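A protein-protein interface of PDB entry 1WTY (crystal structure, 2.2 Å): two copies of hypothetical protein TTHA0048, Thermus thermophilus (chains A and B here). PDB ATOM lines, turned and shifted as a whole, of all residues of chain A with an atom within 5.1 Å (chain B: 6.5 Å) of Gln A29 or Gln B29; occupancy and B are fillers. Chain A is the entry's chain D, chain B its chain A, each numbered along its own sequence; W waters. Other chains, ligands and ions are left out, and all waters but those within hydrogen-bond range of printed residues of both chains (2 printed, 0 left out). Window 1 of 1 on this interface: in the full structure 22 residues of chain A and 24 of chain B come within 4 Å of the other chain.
The side-chain carboxylate of Glu B32 sits close to the side-chain carboxylate of Glu A32, 2.7 Å away.
The backbone carbonyl oxygen of Thr B85 sits at hydrogen-bond distance from the side-chain amide nitrogen of Gln A29.
NE2 of Gln B29 lies within hydrogen-bond range of OE1 of Glu A32 (3.2 Å).
The side-chain hydroxyl of Thr B88 lies within hydrogen-bond range of the side-chain amide nitrogen of Gln A29.
The side-chain carboxylate of Glu B32 lies within hydrogen-bond range of the side-chain amide nitrogen of Gln A29, 3.4 Å away.
The guanidinium group of Arg B10 is in hydrogen-bond range of the backbone carbonyl oxygen of Thr A88.
OD2 of Asp A25 lies within salt-bridge range of NH2 of Arg B10.
The side-chain carboxylate (OD1) of Asp B25 lies within salt-bridge range of the guanidinium group (NE) of Arg A30.
The side-chain hydroxyl of Thr A88 lies within hydrogen-bond range of the side-chain amide nitrogen of Gln B29, 3.1 Å away.
The side-chain carboxylate (OD2) of Asp A25 is in salt-bridge range of the guanidinium group (NE) of Arg B30, 2.7 Å away.
Water W2 lies within hydrogen-bond range of the side-chain amide oxygen (OE1) of Gln B29 (2.7 Å), the side-chain carboxylate (OD1) of Asp A25 (2.7 Å) and the guanidinium group (NH2) of Arg B10 (3.1 Å).
Water W1 lies within hydrogen-bond range of the side-chain carboxylate (OD2) of Asp B25 (2.7 Å) and the side-chain amide oxygen (OE1) of Gln A29 (2.8 Å).
Asp A25 touches Ser B26, and with the chains exchanged Ser A26 touches Asp B25.
Asp A25 touches Gln B29, and with the chains exchanged Gln A29 touches Asp B25.
Gln A29 touches its own counterpart, Gln B29.
Phe A33 touches Thr B88, and with the chains exchanged Thr A88 touches Phe B33.
Of the 21 pairs that touch across the chains among the printed residues, 17 have their exchanged pair printed and touching as well.
Printed residues of chain B within 4 Å of Gln A29: Asp B25, Ile B28, Gln B29, Glu B32, Thr B85 and Thr B88.
Printed residues of chain A within 4 Å of Gln B29: Asp A25 (3.4 Å), Gln A29 (3.5 Å), Glu A32 (3.2 Å), Thr A85 (3.9 Å) and Thr A88 (3.1 Å).
Printed residues of chain B within 4 Å of Thr A85: Gln B29.
Printed residues of chain B within 4 Å of Ser A26: Asp B25 and Ser B26.
Printed residues of chain A within 4 Å of Asn B86: Phe A33 (3.99 Å).
Ala B27 touches none of the printed residues of chain A.
Ile A28 touches none of the printed residues of chain B.
The nearest printed residue of chain A that does not touch Thr B85 is Phe A33 (4.8 Å).
Among the printed residues, merely in contact across the chains: Phe A33 with Thr B88 (3.2 Å), Gln A29 with Asp B25 (3.3 Å), Asp A25 with Gln B29 (3.4 Å), Thr A88 with Phe B33 (3.4 Å), Gln A29 with Gln B29 (3.5 Å), Asp A25 with Ser B26 (3.6 Å), Ser A26 with Ser B26 (3.7 Å), Thr A85 with Gln B29 (3.9 Å), Gln A29 with Ile B28 (3.9 Å), Ser A26 with Asp B25 (3.98 Å) and Phe A33 with Asn B86 (3.99 Å).
The side-chain hydroxyl (OG1) of Thr A85 sits close to the side-chain carboxylate (OE1) of Glu A32 (3.5 Å).
The backbone carbonyl oxygen (O) of Thr A85 is in hydrogen-bond range of the side-chain hydroxyl (OG1) of Thr A88 (3.1 Å).
The backbone carbonyl oxygen of Thr B85 lies within hydrogen-bond range of the side-chain hydroxyl of Thr B88 (2.8 Å).
OG1 of Thr B34 is in hydrogen-bond range of O of Arg B30 (2.8 Å).
The side-chain carboxylate of Glu B32 sits close to the side-chain hydroxyl of Thr B85.
NH2 of Arg B30 sits at hydrogen-bond distance from O of Arg B10 (2.6 Å).
Of the 18 printed residues of chain B, 11 touch a printed residue of chain A.
Hydrophobic or aromatic side chains of chain B that line the printed part of chain A: Ile B28 and Phe B33.
Of the 11 printed residues of chain A, 8 touch a printed residue of chain B.
Printed residues of chain A that touch a printed residue of chain B: Asp A25, Ser A26, Gln A29, Arg A30, Glu A32, Phe A33, Thr A85 and Thr A88.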
ATOM      1  N   ASP A  25     -23.660 -26.901   0.753  1.00  0.00           N
ATOM      2  CA  ASP A  25     -24.467 -27.684  -0.171  1.00  0.00           C
ATOM      3  C   ASP A  25     -25.247 -26.769  -1.132  1.00  0.00           C
ATOM      4  O   ASP A  25     -25.411 -27.090  -2.309  1.00  0.00           O
ATOM      5  CB  ASP A  25     -25.415 -28.620   0.606  1.00  0.00           C
ATOM      6  CG  ASP A  25     -24.678 -29.816   1.261  1.00  0.00           C
ATOM      7  OD1 ASP A  25     -23.465 -30.035   1.004  1.00  0.00           O
ATOM      8  OD2 ASP A  25     -25.325 -30.551   2.029  1.00  0.00           O
ATOM      9  N   SER A  26     -25.704 -25.621  -0.648  1.00  0.00           N
ATOM     10  CA  SER A  26     -26.440 -24.723  -1.526  1.00  0.00           C
ATOM     11  C   SER A  26     -25.478 -24.122  -2.560  1.00  0.00           C
ATOM     12  O   SER A  26     -25.862 -23.882  -3.707  1.00  0.00           O
ATOM     13  CB  SER A  26     -27.129 -23.609  -0.722  1.00  0.00           C
ATOM     14  OG  SER A  26     -26.214 -22.620  -0.284  1.00  0.00           O
ATOM     15  N   ALA A  27     -24.227 -23.893  -2.166  1.00  0.00           N
ATOM     16  CA  ALA A  27     -23.252 -23.333  -3.097  1.00  0.00           C
ATOM     17  C   ALA A  27     -22.957 -24.366  -4.182  1.00  0.00           C
ATOM     18  O   ALA A  27     -22.831 -24.024  -5.358  1.00  0.00           O
ATOM     19  CB  ALA A  27     -21.975 -22.947  -2.365  1.00  0.00           C
ATOM     20  N   ILE A  28     -22.861 -25.631  -3.787  1.00  0.00           N
ATOM     21  CA  ILE A  28     -22.597 -26.705  -4.739  1.00  0.00           C
ATOM     22  C   ILE A  28     -23.754 -26.892  -5.732  1.00  0.00           C
ATOM     23  O   ILE A  28     -23.537 -27.119  -6.925  1.00  0.00           O
ATOM     24  CB  ILE A  28     -22.358 -28.052  -4.012  1.00  0.00           C
ATOM     25  CG1 ILE A  28     -21.041 -27.996  -3.240  1.00  0.00           C
ATOM     26  CG2 ILE A  28     -22.347 -29.196  -5.017  1.00  0.00           C
ATOM     27  CD1 ILE A  28     -20.740 -29.253  -2.449  1.00  0.00           C
ATOM     28  N   GLN A  29     -24.982 -26.816  -5.237  1.00  0.00           N
ATOM     29  CA  GLN A  29     -26.144 -26.980  -6.098  1.00  0.00           C
ATOM     30  C   GLN A  29     -26.154 -25.847  -7.119  1.00  0.00           C
ATOM     31  O   GLN A  29     -26.460 -26.059  -8.287  1.00  0.00           O
ATOM     32  CB  GLN A  29     -27.418 -26.946  -5.251  1.00  0.00           C
ATOM     33  CG  GLN A  29     -28.627 -27.672  -5.837  1.00  0.00           C
ATOM     34  CD  GLN A  29     -29.300 -26.912  -6.957  1.00  0.00           C
ATOM     35  OE1 GLN A  29     -29.527 -25.701  -6.856  1.00  0.00           O
ATOM     36  NE2 GLN A  29     -29.639 -27.618  -8.031  1.00  0.00           N
ATOM     37  N   ARG A  30     -25.793 -24.648  -6.678  1.00  0.00           N
ATOM     38  CA  ARG A  30     -25.784 -23.484  -7.558  1.00  0.00           C
ATOM     39  C   ARG A  30     -24.680 -23.544  -8.608  1.00  0.00           C
ATOM     40  O   ARG A  30     -24.840 -23.042  -9.728  1.00  0.00           O
ATOM     41  CB  ARG A  30     -25.675 -22.220  -6.716  1.00  0.00           C
ATOM     42  CG  ARG A  30     -26.874 -22.063  -5.797  1.00  0.00           C
ATOM     43  CD  ARG A  30     -26.800 -20.832  -4.932  1.00  0.00           C
ATOM     44  NE  ARG A  30     -28.060 -20.660  -4.233  1.00  0.00           N
ATOM     45  CZ  ARG A  30     -28.480 -19.519  -3.710  1.00  0.00           C
ATOM     46  NH1 ARG A  30     -27.730 -18.430  -3.803  1.00  0.00           N
ATOM     47  NH2 ARG A  30     -29.657 -19.470  -3.101  1.00  0.00           N
ATOM     48  N   PHE A  31     -23.568 -24.173  -8.246  1.00  0.00           N
ATOM     49  CA  PHE A  31     -22.457 -24.329  -9.163  1.00  0.00           C
ATOM     50  C   PHE A  31     -22.872 -25.331 -10.236  1.00  0.00           C
ATOM     51  O   PHE A  31     -22.406 -25.267 -11.374  1.00  0.00           O
ATOM     52  CB  PHE A  31     -21.230 -24.848  -8.419  1.00  0.00           C
ATOM     53  CG  PHE A  31     -20.240 -25.536  -9.304  1.00  0.00           C
ATOM     54  CD1 PHE A  31     -19.494 -24.815 -10.219  1.00  0.00           C
ATOM     55  CD2 PHE A  31     -20.070 -26.916  -9.231  1.00  0.00           C
ATOM     56  CE1 PHE A  31     -18.588 -25.456 -11.053  1.00  0.00           C
ATOM     57  CE2 PHE A  31     -19.170 -27.566 -10.056  1.00  0.00           C
ATOM     58  CZ  PHE A  31     -18.425 -26.837 -10.972  1.00  0.00           C
ATOM     59  N   GLU A  32     -23.753 -26.256  -9.861  1.00  0.00           N
ATOM     60  CA  GLU A  32     -24.238 -27.271 -10.785  1.00  0.00           C
ATOM     61  C   GLU A  32     -25.067 -26.654 -11.891  1.00  0.00           C
ATOM     62  O   GLU A  32     -24.791 -26.885 -13.066  1.00  0.00           O
ATOM     63  CB  GLU A  32     -25.091 -28.326 -10.067  1.00  0.00           C
ATOM     64  CG  GLU A  32     -24.326 -29.234  -9.104  1.00  0.00           C
ATOM     65  CD  GLU A  32     -25.242 -30.193  -8.343  1.00  0.00           C
ATOM     66  OE1 GLU A  32     -24.764 -30.863  -7.403  1.00  0.00           O
ATOM     67  OE2 GLU A  32     -26.441 -30.283  -8.684  1.00  0.00           O
ATOM     68  N   PHE A  33     -26.083 -25.869 -11.535  1.00  0.00           N
ATOM     69  CA  PHE A  33     -26.899 -25.290 -12.585  1.00  0.00           C
ATOM     70  C   PHE A  33     -26.174 -24.196 -13.355  1.00  0.00           C
ATOM     71  O   PHE A  33     -26.404 -24.030 -14.548  1.00  0.00           O
ATOM     72  CB  PHE A  33     -28.285 -24.828 -12.059  1.00  0.00           C
ATOM     73  CG  PHE A  33     -28.263 -23.645 -11.113  1.00  0.00           C
ATOM     74  CD1 PHE A  33     -27.757 -22.412 -11.508  1.00  0.00           C
ATOM     75  CD2 PHE A  33     -28.831 -23.751  -9.844  1.00  0.00           C
ATOM     76  CE1 PHE A  33     -27.817 -21.303 -10.657  1.00  0.00           C
ATOM     77  CE2 PHE A  33     -28.895 -22.648  -8.988  1.00  0.00           C
ATOM     78  CZ  PHE A  33     -28.385 -21.421  -9.400  1.00  0.00           C
ATOM     79  N   THR A  85     -20.209 -33.904  -8.460  1.00  0.00           N
ATOM     80  CA  THR A  85     -21.334 -33.469  -7.654  1.00  0.00           C
ATOM     81  C   THR A  85     -22.429 -34.526  -7.553  1.00  0.00           C
ATOM     82  O   THR A  85     -23.382 -34.367  -6.794  1.00  0.00           O
ATOM     83  CB  THR A  85     -21.930 -32.126  -8.170  1.00  0.00           C
ATOM     84  OG1 THR A  85     -22.415 -32.278  -9.508  1.00  0.00           O
ATOM     85  CG2 THR A  85     -20.869 -31.048  -8.142  1.00  0.00           C
ATOM     86  N   THR A  88     -21.818 -36.512  -4.011  1.00  0.00           N
ATOM     87  CA  THR A  88     -21.649 -35.748  -2.792  1.00  0.00           C
ATOM     88  C   THR A  88     -22.287 -36.370  -1.557  1.00  0.00           C
ATOM     89  O   THR A  88     -22.435 -35.719  -0.533  1.00  0.00           O
ATOM     90  CB  THR A  88     -22.113 -34.293  -2.972  1.00  0.00           C
ATOM     91  OG1 THR A  88     -23.375 -34.255  -3.658  1.00  0.00           O
ATOM     92  CG2 THR A  88     -21.056 -33.522  -3.767  1.00  0.00           C
ATOM     93  N   ARG B  10     -29.331 -36.369   6.152  1.00  0.00           N
ATOM     94  CA  ARG B  10     -28.910 -35.056   5.693  1.00  0.00           C
ATOM     95  C   ARG B  10     -30.072 -34.330   5.028  1.00  0.00           C
ATOM     96  O   ARG B  10     -30.259 -33.147   5.251  1.00  0.00           O
ATOM     97  CB  ARG B  10     -27.730 -35.180   4.723  1.00  0.00           C
ATOM     98  CG  ARG B  10     -26.421 -35.550   5.413  1.00  0.00           C
ATOM     99  CD  ARG B  10     -25.296 -35.724   4.414  1.00  0.00           C
ATOM    100  NE  ARG B  10     -24.976 -34.487   3.711  1.00  0.00           N
ATOM    101  CZ  ARG B  10     -24.192 -34.428   2.639  1.00  0.00           C
ATOM    102  NH1 ARG B  10     -23.659 -35.546   2.163  1.00  0.00           N
ATOM    103  NH2 ARG B  10     -23.939 -33.259   2.042  1.00  0.00           N
ATOM    104  N   ARG B  24     -33.255 -23.933   0.852  1.00  0.00           N
ATOM    105  CA  ARG B  24     -33.984 -24.515  -0.268  1.00  0.00           C
ATOM    106  C   ARG B  24     -33.051 -25.263  -1.210  1.00  0.00           C
ATOM    107  O   ARG B  24     -33.236 -26.453  -1.497  1.00  0.00           O
ATOM    108  CB  ARG B  24     -34.703 -23.426  -1.062  1.00  0.00           C
ATOM    109  CG  ARG B  24     -35.471 -23.957  -2.265  1.00  0.00           C
ATOM    110  CD  ARG B  24     -35.809 -22.821  -3.210  1.00  0.00           C
ATOM    111  NE  ARG B  24     -34.588 -22.247  -3.760  1.00  0.00           N
ATOM    112  CZ  ARG B  24     -34.449 -20.983  -4.141  1.00  0.00           C
ATOM    113  NH1 ARG B  24     -33.284 -20.572  -4.623  1.00  0.00           N
ATOM    114  NH2 ARG B  24     -35.465 -20.136  -4.040  1.00  0.00           N
ATOM    115  N   ASP B  25     -32.035 -24.556  -1.684  1.00  0.00           N
ATOM    116  CA  ASP B  25     -31.103 -25.147  -2.620  1.00  0.00           C
ATOM    117  C   ASP B  25     -30.286 -26.327  -2.054  1.00  0.00           C
ATOM    118  O   ASP B  25     -29.960 -27.256  -2.797  1.00  0.00           O
ATOM    119  CB  ASP B  25     -30.206 -24.043  -3.204  1.00  0.00           C
ATOM    120  CG  ASP B  25     -30.990 -23.047  -4.106  1.00  0.00           C
ATOM    121  OD1 ASP B  25     -30.403 -22.030  -4.533  1.00  0.00           O
ATOM    122  OD2 ASP B  25     -32.185 -23.275  -4.397  1.00  0.00           O
ATOM    123  N   SER B  26     -29.966 -26.320  -0.759  1.00  0.00           N
ATOM    124  CA  SER B  26     -29.216 -27.456  -0.185  1.00  0.00           C
ATOM    125  C   SER B  26     -30.140 -28.677  -0.011  1.00  0.00           C
ATOM    126  O   SER B  26     -29.676 -29.828   0.004  1.00  0.00           O
ATOM    127  CB  SER B  26     -28.584 -27.092   1.164  1.00  0.00           C
ATOM    128  OG  SER B  26     -29.569 -26.816   2.151  1.00  0.00           O
ATOM    129  N   ALA B  27     -31.441 -28.436   0.135  1.00  0.00           N
ATOM    130  CA  ALA B  27     -32.383 -29.542   0.263  1.00  0.00           C
ATOM    131  C   ALA B  27     -32.481 -30.183  -1.122  1.00  0.00           C
ATOM    132  O   ALA B  27     -32.459 -31.400  -1.254  1.00  0.00           O
ATOM    133  CB  ALA B  27     -33.737 -29.046   0.728  1.00  0.00           C
ATOM    134  N   ILE B  28     -32.567 -29.359  -2.161  1.00  0.00           N
ATOM    135  CA  ILE B  28     -32.612 -29.884  -3.525  1.00  0.00           C
ATOM    136  C   ILE B  28     -31.335 -30.682  -3.804  1.00  0.00           C
ATOM    137  O   ILE B  28     -31.377 -31.759  -4.407  1.00  0.00           O
ATOM    138  CB  ILE B  28     -32.712 -28.743  -4.555  1.00  0.00           C
ATOM    139  CG1 ILE B  28     -34.057 -28.015  -4.378  1.00  0.00           C
ATOM    140  CG2 ILE B  28     -32.530 -29.296  -5.967  1.00  0.00           C
ATOM    141  CD1 ILE B  28     -34.203 -26.709  -5.170  1.00  0.00           C
ATOM    142  N   GLN B  29     -30.204 -30.150  -3.351  1.00  0.00           N
ATOM    143  CA  GLN B  29     -28.902 -30.778  -3.548  1.00  0.00           C
ATOM    144  C   GLN B  29     -28.850 -32.128  -2.833  1.00  0.00           C
ATOM    145  O   GLN B  29     -28.292 -33.103  -3.356  1.00  0.00           O
ATOM    146  CB  GLN B  29     -27.803 -29.850  -3.013  1.00  0.00           C
ATOM    147  CG  GLN B  29     -26.467 -29.945  -3.729  1.00  0.00           C
ATOM    148  CD  GLN B  29     -25.678 -31.183  -3.369  1.00  0.00           C
ATOM    149  OE1 GLN B  29     -25.431 -31.459  -2.198  1.00  0.00           O
ATOM    150  NE2 GLN B  29     -25.267 -31.931  -4.378  1.00  0.00           N
ATOM    151  N   ARG B  30     -29.440 -32.184  -1.643  1.00  0.00           N
ATOM    152  CA  ARG B  30     -29.466 -33.420  -0.872  1.00  0.00           C
ATOM    153  C   ARG B  30     -30.423 -34.445  -1.469  1.00  0.00           C
ATOM    154  O   ARG B  30     -30.209 -35.660  -1.350  1.00  0.00           O
ATOM    155  CB  ARG B  30     -29.803 -33.105   0.586  1.00  0.00           C
ATOM    156  CG  ARG B  30     -28.610 -32.457   1.259  1.00  0.00           C
ATOM    157  CD  ARG B  30     -28.906 -31.804   2.585  1.00  0.00           C
ATOM    158  NE  ARG B  30     -27.661 -31.252   3.102  1.00  0.00           N
ATOM    159  CZ  ARG B  30     -27.379 -31.094   4.389  1.00  0.00           C
ATOM    160  NH1 ARG B  30     -26.208 -30.583   4.742  1.00  0.00           N
ATOM    161  NH2 ARG B  30     -28.257 -31.461   5.316  1.00  0.00           N
ATOM    162  N   PHE B  31     -31.477 -33.960  -2.114  1.00  0.00           N
ATOM    163  CA  PHE B  31     -32.419 -34.849  -2.770  1.00  0.00           C
ATOM    164  C   PHE B  31     -31.669 -35.503  -3.925  1.00  0.00           C
ATOM    165  O   PHE B  31     -31.871 -36.678  -4.213  1.00  0.00           O
ATOM    166  CB  PHE B  31     -33.618 -34.075  -3.319  1.00  0.00           C
ATOM    167  CG  PHE B  31     -34.371 -34.813  -4.400  1.00  0.00           C
ATOM    168  CD1 PHE B  31     -35.137 -35.930  -4.097  1.00  0.00           C
ATOM    169  CD2 PHE B  31     -34.289 -34.399  -5.728  1.00  0.00           C
ATOM    170  CE1 PHE B  31     -35.813 -36.625  -5.099  1.00  0.00           C
ATOM    171  CE2 PHE B  31     -34.963 -35.090  -6.741  1.00  0.00           C
ATOM    172  CZ  PHE B  31     -35.725 -36.202  -6.424  1.00  0.00           C
ATOM    173  N   GLU B  32     -30.793 -34.741  -4.572  1.00  0.00           N
ATOM    174  CA  GLU B  32     -30.023 -35.263  -5.694  1.00  0.00           C
ATOM    175  C   GLU B  32     -29.131 -36.457  -5.391  1.00  0.00           C
ATOM    176  O   GLU B  32     -29.229 -37.469  -6.074  1.00  0.00           O
ATOM    177  CB  GLU B  32     -29.147 -34.183  -6.312  1.00  0.00           C
ATOM    178  CG  GLU B  32     -29.858 -33.199  -7.199  1.00  0.00           C
ATOM    179  CD  GLU B  32     -28.896 -32.173  -7.769  1.00  0.00           C
ATOM    180  OE1 GLU B  32     -29.137 -30.959  -7.580  1.00  0.00           O
ATOM    181  OE2 GLU B  32     -27.896 -32.583  -8.405  1.00  0.00           O
ATOM    182  N   PHE B  33     -28.236 -36.349  -4.408  1.00  0.00           N
ATOM    183  CA  PHE B  33     -27.368 -37.485  -4.123  1.00  0.00           C
ATOM    184  C   PHE B  33     -28.099 -38.603  -3.393  1.00  0.00           C
ATOM    185  O   PHE B  33     -27.715 -39.770  -3.508  1.00  0.00           O
ATOM    186  CB  PHE B  33     -26.081 -37.075  -3.364  1.00  0.00           C
ATOM    187  CG  PHE B  33     -26.306 -36.486  -1.998  1.00  0.00           C
ATOM    188  CD1 PHE B  33     -26.037 -35.141  -1.755  1.00  0.00           C
ATOM    189  CD2 PHE B  33     -26.743 -37.276  -0.941  1.00  0.00           C
ATOM    190  CE1 PHE B  33     -26.195 -34.593  -0.480  1.00  0.00           C
ATOM    191  CE2 PHE B  33     -26.905 -36.733   0.340  1.00  0.00           C
ATOM    192  CZ  PHE B  33     -26.628 -35.388   0.563  1.00  0.00           C
ATOM    193  N   THR B  34     -29.155 -38.267  -2.656  1.00  0.00           N
ATOM    194  CA  THR B  34     -29.912 -39.299  -1.964  1.00  0.00           C
ATOM    195  C   THR B  34     -30.635 -40.154  -3.009  1.00  0.00           C
ATOM    196  O   THR B  34     -30.623 -41.385  -2.915  1.00  0.00           O
ATOM    197  CB  THR B  34     -30.901 -38.685  -0.949  1.00  0.00           C
ATOM    198  OG1 THR B  34     -30.155 -38.085   0.113  1.00  0.00           O
ATOM    199  CG2 THR B  34     -31.796 -39.737  -0.345  1.00  0.00           C
ATOM    200  N   THR B  85     -33.514 -31.076 -11.543  1.00  0.00           N
ATOM    201  CA  THR B  85     -32.607 -30.332 -10.667  1.00  0.00           C
ATOM    202  C   THR B  85     -31.479 -29.668 -11.438  1.00  0.00           C
ATOM    203  O   THR B  85     -30.919 -28.669 -10.994  1.00  0.00           O
ATOM    204  CB  THR B  85     -31.964 -31.240  -9.589  1.00  0.00           C
ATOM    205  OG1 THR B  85     -31.036 -32.139 -10.204  1.00  0.00           O
ATOM    206  CG2 THR B  85     -33.028 -32.039  -8.860  1.00  0.00           C
ATOM    207  N   ASN B  86     -31.152 -30.226 -12.596  1.00  0.00           N
ATOM    208  CA  ASN B  86     -30.078 -29.695 -13.415  1.00  0.00           C
ATOM    209  C   ASN B  86     -30.417 -28.371 -14.076  1.00  0.00           C
ATOM    210  O   ASN B  86     -29.531 -27.677 -14.567  1.00  0.00           O
ATOM    211  CB  ASN B  86     -29.691 -30.701 -14.493  1.00  0.00           C
ATOM    212  CG  ASN B  86     -28.257 -30.535 -14.939  1.00  0.00           C
ATOM    213  OD1 ASN B  86     -27.847 -29.453 -15.351  1.00  0.00           O
ATOM    214  ND2 ASN B  86     -27.480 -31.610 -14.855  1.00  0.00           N
ATOM    215  N   HIS B  87     -31.698 -28.020 -14.090  1.00  0.00           N
ATOM    216  CA  HIS B  87     -32.143 -26.771 -14.705  1.00  0.00           C
ATOM    217  C   HIS B  87     -32.691 -25.779 -13.688  1.00  0.00           C
ATOM    218  O   HIS B  87     -33.525 -24.942 -14.033  1.00  0.00           O
ATOM    219  CB  HIS B  87     -33.224 -27.065 -15.748  1.00  0.00           C
ATOM    220  CG  HIS B  87     -32.782 -28.014 -16.813  1.00  0.00           C
ATOM    221  ND1 HIS B  87     -31.757 -27.723 -17.688  1.00  0.00           N
ATOM    222  CD2 HIS B  87     -33.190 -29.268 -17.114  1.00  0.00           C
ATOM    223  CE1 HIS B  87     -31.551 -28.760 -18.479  1.00  0.00           C
ATOM    224  NE2 HIS B  87     -32.407 -29.711 -18.151  1.00  0.00           N
ATOM    225  N   THR B  88     -32.223 -25.866 -12.446  1.00  0.00           N
ATOM    226  CA  THR B  88     -32.705 -24.980 -11.394  1.00  0.00           C
ATOM    227  C   THR B  88     -32.244 -23.531 -11.452  1.00  0.00           C
ATOM    228  O   THR B  88     -32.482 -22.779 -10.509  1.00  0.00           O
ATOM    229  CB  THR B  88     -32.386 -25.528  -9.985  1.00  0.00           C
ATOM    230  OG1 THR B  88     -31.058 -26.063  -9.962  1.00  0.00           O
ATOM    231  CG2 THR B  88     -33.390 -26.601  -9.593  1.00  0.00           C
ATOM    232  N   ALA B  94     -37.094 -24.421  -9.072  1.00  0.00           N
ATOM    233  CA  ALA B  94     -36.464 -24.800  -7.811  1.00  0.00           C
ATOM    234  C   ALA B  94     -37.504 -24.799  -6.702  1.00  0.00           C
ATOM    235  O   ALA B  94     -37.447 -25.628  -5.794  1.00  0.00           O
ATOM    236  CB  ALA B  94     -35.328 -23.844  -7.469  1.00  0.00           C
ATOM    237  N   LEU B 101     -40.194 -32.295  -1.940  1.00  0.00           N
ATOM    238  CA  LEU B 101     -39.238 -33.052  -1.143  1.00  0.00           C
ATOM    239  C   LEU B 101     -39.784 -33.735   0.102  1.00  0.00           C
ATOM    240  O   LEU B 101     -39.373 -34.853   0.419  1.00  0.00           O
ATOM    241  CB  LEU B 101     -38.036 -32.180  -0.789  1.00  0.00           C
ATOM    242  CG  LEU B 101     -37.334 -31.683  -2.056  1.00  0.00           C
ATOM    243  CD1 LEU B 101     -36.138 -30.820  -1.699  1.00  0.00           C
ATOM    244  CD2 LEU B 101     -36.909 -32.874  -2.894  1.00  0.00           C
HETATM  245  O   HOH W   1     -31.812 -24.049  -6.984  1.00  0.00           O
HETATM  246  O   HOH W   2     -23.318 -32.089  -0.727  1.00  0.00           O
